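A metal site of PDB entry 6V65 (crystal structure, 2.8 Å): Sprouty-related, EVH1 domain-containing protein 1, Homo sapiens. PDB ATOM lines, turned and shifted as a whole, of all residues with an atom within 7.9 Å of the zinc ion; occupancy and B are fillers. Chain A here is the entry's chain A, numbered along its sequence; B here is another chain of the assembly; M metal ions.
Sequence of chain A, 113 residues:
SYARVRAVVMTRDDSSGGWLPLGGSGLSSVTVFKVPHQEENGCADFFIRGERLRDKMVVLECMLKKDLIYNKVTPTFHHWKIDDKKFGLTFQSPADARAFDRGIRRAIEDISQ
The backbone carbonyl oxygen (O) of Ala 44 lies close to a ring nitrogen (NE2) of His 37.
OD1 of Asp 45 is in hydrogen-bond range of NE2 of His 37 (2.7 Å).
O of His 37 is in hydrogen-bond range of ND2 of Asn 178 of chain B, at 2.9 Å.
Four residues have an atom within 4 Å of the zinc ion: His 37, Cys 43, His 230 of chain B and Asp 251 of chain B.
The zinc ion is bound by ND1 of His 37 (2.0 Å), OD1 of Asp 251 of chain B (2.1 Å), SG of Cys 43 (2.3 Å) and NE2 of His 230 of chain B (2.6 Å).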
ATOM      1  N   VAL A  35      -8.972  28.259  22.278  1.00  0.00           N
ATOM      2  CA  VAL A  35      -7.687  27.715  21.856  1.00  0.00           C
ATOM      3  C   VAL A  35      -7.679  27.674  20.326  1.00  0.00           C
ATOM      4  O   VAL A  35      -8.477  26.934  19.741  1.00  0.00           O
ATOM      5  CB  VAL A  35      -7.424  26.331  22.472  1.00  0.00           C
ATOM      6  CG1 VAL A  35      -6.164  25.717  21.875  1.00  0.00           C
ATOM      7  CG2 VAL A  35      -7.307  26.448  23.980  1.00  0.00           C
ATOM      8  N   PRO A  36      -6.820  28.444  19.665  1.00  0.00           N
ATOM      9  CA  PRO A  36      -6.871  28.484  18.195  1.00  0.00           C
ATOM     10  C   PRO A  36      -6.481  27.146  17.592  1.00  0.00           C
ATOM     11  O   PRO A  36      -5.572  26.468  18.069  1.00  0.00           O
ATOM     12  CB  PRO A  36      -5.861  29.586  17.835  1.00  0.00           C
ATOM     13  CG  PRO A  36      -4.919  29.612  18.990  1.00  0.00           C
ATOM     14  CD  PRO A  36      -5.737  29.273  20.205  1.00  0.00           C
ATOM     15  N   HIS A  37      -7.214  26.768  16.533  1.00  0.00           N
ATOM     16  CA  HIS A  37      -6.875  25.545  15.801  1.00  0.00           C
ATOM     17  C   HIS A  37      -5.508  25.659  15.144  1.00  0.00           C
ATOM     18  O   HIS A  37      -4.652  24.782  15.296  1.00  0.00           O
ATOM     19  CB  HIS A  37      -7.946  25.245  14.748  1.00  0.00           C
ATOM     20  CG  HIS A  37      -9.259  24.796  15.323  1.00  0.00           C
ATOM     21  ND1 HIS A  37     -10.359  24.551  14.545  1.00  0.00           N
ATOM     22  CD2 HIS A  37      -9.639  24.543  16.593  1.00  0.00           C
ATOM     23  CE1 HIS A  37     -11.364  24.167  15.310  1.00  0.00           C
ATOM     24  NE2 HIS A  37     -10.951  24.156  16.559  1.00  0.00           N
ATOM     25  N   GLN A  38      -5.269  26.744  14.408  1.00  0.00           N
ATOM     26  CA  GLN A  38      -3.977  26.969  13.775  1.00  0.00           C
ATOM     27  C   GLN A  38      -3.432  28.348  14.126  1.00  0.00           C
ATOM     28  O   GLN A  38      -2.790  28.522  15.164  1.00  0.00           O
ATOM     29  CB  GLN A  38      -4.079  26.790  12.261  1.00  0.00           C
ATOM     30  CG  GLN A  38      -3.981  25.347  11.783  1.00  0.00           C
ATOM     31  CD  GLN A  38      -2.598  24.758  11.958  1.00  0.00           C
ATOM     32  OE1 GLN A  38      -1.655  25.458  12.317  1.00  0.00           O
ATOM     33  NE2 GLN A  38      -2.471  23.460  11.697  1.00  0.00           N
ATOM     34  N   GLY A  42      -7.739  32.759  13.921  1.00  0.00           N
ATOM     35  CA  GLY A  42      -8.432  31.811  13.082  1.00  0.00           C
ATOM     36  C   GLY A  42      -9.470  30.994  13.830  1.00  0.00           C
ATOM     37  O   GLY A  42      -9.823  31.328  14.958  1.00  0.00           O
ATOM     38  N   CYS A  43      -9.961  29.923  13.202  1.00  0.00           N
ATOM     39  CA  CYS A  43     -10.910  29.035  13.849  1.00  0.00           C
ATOM     40  C   CYS A  43     -10.312  28.457  15.133  1.00  0.00           C
ATOM     41  O   CYS A  43      -9.094  28.299  15.257  1.00  0.00           O
ATOM     42  CB  CYS A  43     -11.331  27.910  12.896  1.00  0.00           C
ATOM     43  SG  CYS A  43      -9.991  27.149  11.926  1.00  0.00           S
ATOM     44  N   ALA A  44     -11.182  28.151  16.094  1.00  0.00           N
ATOM     45  CA  ALA A  44     -10.727  27.764  17.423  1.00  0.00           C
ATOM     46  C   ALA A  44     -11.766  26.876  18.097  1.00  0.00           C
ATOM     47  O   ALA A  44     -12.887  26.714  17.615  1.00  0.00           O
ATOM     48  CB  ALA A  44     -10.437  28.991  18.296  1.00  0.00           C
ATOM     49  N   ASP A  45     -11.367  26.310  19.234  1.00  0.00           N
ATOM     50  CA  ASP A  45     -12.266  25.619  20.153  1.00  0.00           C
ATOM     51  C   ASP A  45     -12.453  26.462  21.401  1.00  0.00           C
ATOM     52  O   ASP A  45     -11.572  27.226  21.794  1.00  0.00           O
ATOM     53  CB  ASP A  45     -11.717  24.246  20.524  1.00  0.00           C
ATOM     54  CG  ASP A  45     -11.755  23.260  19.378  1.00  0.00           C
ATOM     55  OD1 ASP A  45     -12.664  23.371  18.537  1.00  0.00           O
ATOM     56  OD2 ASP A  45     -10.869  22.385  19.314  1.00  0.00           O
ATOM     57  N   ILE A 111     -18.002  30.801  17.332  1.00  0.00           N
ATOM     58  CA  ILE A 111     -17.677  29.410  17.051  1.00  0.00           C
ATOM     59  C   ILE A 111     -17.377  29.223  15.562  1.00  0.00           C
ATOM     60  O   ILE A 111     -16.315  28.728  15.188  1.00  0.00           O
ATOM     61  CB  ILE A 111     -18.794  28.474  17.530  1.00  0.00           C
ATOM     62  CG1 ILE A 111     -18.746  28.339  19.060  1.00  0.00           C
ATOM     63  CG2 ILE A 111     -18.678  27.112  16.867  1.00  0.00           C
ATOM     64  CD1 ILE A 111     -19.704  27.324  19.629  1.00  0.00           C
ATOM     65  N   SER A 112     -18.319  29.609  14.701  1.00  0.00           N
ATOM     66  CA  SER A 112     -18.127  29.474  13.259  1.00  0.00           C
ATOM     67  C   SER A 112     -18.240  28.015  12.812  1.00  0.00           C
ATOM     68  O   SER A 112     -17.429  27.166  13.197  1.00  0.00           O
ATOM     69  N   ASN B 178      -4.260  20.707  20.284  1.00  0.00           N
ATOM     70  CA  ASN B 178      -4.648  20.215  18.964  1.00  0.00           C
ATOM     71  C   ASN B 178      -4.181  18.771  18.726  1.00  0.00           C
ATOM     72  O   ASN B 178      -3.835  18.395  17.611  1.00  0.00           O
ATOM     73  CB  ASN B 178      -4.121  21.129  17.847  1.00  0.00           C
ATOM     74  CG  ASN B 178      -4.693  22.535  17.924  1.00  0.00           C
ATOM     75  OD1 ASN B 178      -5.900  22.721  18.086  1.00  0.00           O
ATOM     76  ND2 ASN B 178      -3.814  23.526  17.820  1.00  0.00           N
ATOM     77  N   HIS B 230      -6.233  19.777   7.970  1.00  0.00           N
ATOM     78  CA  HIS B 230      -6.500  21.168   8.314  1.00  0.00           C
ATOM     79  C   HIS B 230      -5.447  22.108   7.708  1.00  0.00           C
ATOM     80  O   HIS B 230      -4.995  23.053   8.348  1.00  0.00           O
ATOM     81  CB  HIS B 230      -6.593  21.361   9.828  1.00  0.00           C
ATOM     82  CG  HIS B 230      -7.389  22.560  10.237  1.00  0.00           C
ATOM     83  ND1 HIS B 230      -6.863  23.827  10.275  1.00  0.00           N
ATOM     84  CD2 HIS B 230      -8.679  22.677  10.634  1.00  0.00           C
ATOM     85  CE1 HIS B 230      -7.788  24.681  10.669  1.00  0.00           C
ATOM     86  NE2 HIS B 230      -8.900  24.010  10.892  1.00  0.00           N
ATOM     87  N   LYS B 247     -11.571  24.960   3.230  1.00  0.00           N
ATOM     88  CA  LYS B 247     -11.524  25.845   4.392  1.00  0.00           C
ATOM     89  C   LYS B 247     -12.834  25.815   5.152  1.00  0.00           C
ATOM     90  O   LYS B 247     -12.847  26.029   6.370  1.00  0.00           O
ATOM     91  CB  LYS B 247     -11.188  27.265   3.955  1.00  0.00           C
ATOM     92  CG  LYS B 247     -10.822  28.200   5.088  1.00  0.00           C
ATOM     93  CD  LYS B 247     -10.645  29.630   4.582  1.00  0.00           C
ATOM     94  CE  LYS B 247     -10.117  30.552   5.669  1.00  0.00           C
ATOM     95  NZ  LYS B 247      -8.731  30.176   6.068  1.00  0.00           N
ATOM     96  N   ASN B 249     -14.962  23.130   5.376  1.00  0.00           N
ATOM     97  CA  ASN B 249     -15.198  21.824   5.984  1.00  0.00           C
ATOM     98  C   ASN B 249     -14.114  21.428   6.981  1.00  0.00           C
ATOM     99  O   ASN B 249     -14.083  20.272   7.414  1.00  0.00           O
ATOM    100  CB  ASN B 249     -15.336  20.759   4.911  1.00  0.00           C
ATOM    101  CG  ASN B 249     -16.581  20.936   4.069  1.00  0.00           C
ATOM    102  OD1 ASN B 249     -17.547  21.572   4.502  1.00  0.00           O
ATOM    103  ND2 ASN B 249     -16.582  20.378   2.868  1.00  0.00           N
ATOM    104  N   PHE B 250     -13.224  22.352   7.359  1.00  0.00           N
ATOM    105  CA  PHE B 250     -12.225  22.078   8.389  1.00  0.00           C
ATOM    106  C   PHE B 250     -12.858  21.519   9.656  1.00  0.00           C
ATOM    107  O   PHE B 250     -12.614  20.366  10.049  1.00  0.00           O
ATOM    108  CB  PHE B 250     -11.447  23.352   8.717  1.00  0.00           C
ATOM    109  CG  PHE B 250     -10.289  23.622   7.810  1.00  0.00           C
ATOM    110  CD1 PHE B 250      -9.784  22.625   6.993  1.00  0.00           C
ATOM    111  CD2 PHE B 250      -9.702  24.872   7.778  1.00  0.00           C
ATOM    112  CE1 PHE B 250      -8.714  22.881   6.147  1.00  0.00           C
ATOM    113  CE2 PHE B 250      -8.629  25.131   6.942  1.00  0.00           C
ATOM    114  CZ  PHE B 250      -8.137  24.141   6.125  1.00  0.00           C
ATOM    115  N   ASP B 251     -13.678  22.320  10.331  1.00  0.00           N
ATOM    116  CA  ASP B 251     -14.150  21.988  11.662  1.00  0.00           C
ATOM    117  C   ASP B 251     -15.279  20.959  11.664  1.00  0.00           C
ATOM    118  O   ASP B 251     -15.544  20.368  12.715  1.00  0.00           O
ATOM    119  CB  ASP B 251     -14.610  23.256  12.383  1.00  0.00           C
ATOM    120  CG  ASP B 251     -13.558  24.336  12.338  1.00  0.00           C
ATOM    121  OD1 ASP B 251     -12.353  23.985  12.297  1.00  0.00           O
ATOM    122  OD2 ASP B 251     -13.926  25.530  12.335  1.00  0.00           O
ATOM    123  N   ALA B 252     -15.931  20.727  10.527  1.00  0.00           N
ATOM    124  CA  ALA B 252     -16.906  19.643  10.454  1.00  0.00           C
ATOM    125  C   ALA B 252     -16.221  18.288  10.627  1.00  0.00           C
ATOM    126  O   ALA B 252     -16.720  17.433  11.363  1.00  0.00           O
ATOM    127  CB  ALA B 252     -17.668  19.698   9.128  1.00  0.00           C
ATOM    128  N   ARG B 254     -13.273  18.047  12.091  1.00  0.00           N
ATOM    129  CA  ARG B 254     -12.701  18.130  13.433  1.00  0.00           C
ATOM    130  C   ARG B 254     -13.715  17.692  14.489  1.00  0.00           C
ATOM    131  O   ARG B 254     -13.344  17.052  15.484  1.00  0.00           O
ATOM    132  CB  ARG B 254     -12.200  19.549  13.695  1.00  0.00           C
ATOM    133  CG  ARG B 254     -11.771  19.821  15.123  1.00  0.00           C
ATOM    134  CD  ARG B 254     -10.357  20.345  15.195  1.00  0.00           C
ATOM    135  NE  ARG B 254     -10.010  20.748  16.559  1.00  0.00           N
ATOM    136  CZ  ARG B 254      -8.785  21.113  16.942  1.00  0.00           C
ATOM    137  NH1 ARG B 254      -7.794  21.113  16.068  1.00  0.00           N
ATOM    138  NH2 ARG B 254      -8.571  21.471  18.195  1.00  0.00           N
HETATM  139 ZN    ZN M   1     -10.577  24.987  12.558  1.00  0.00          ZN
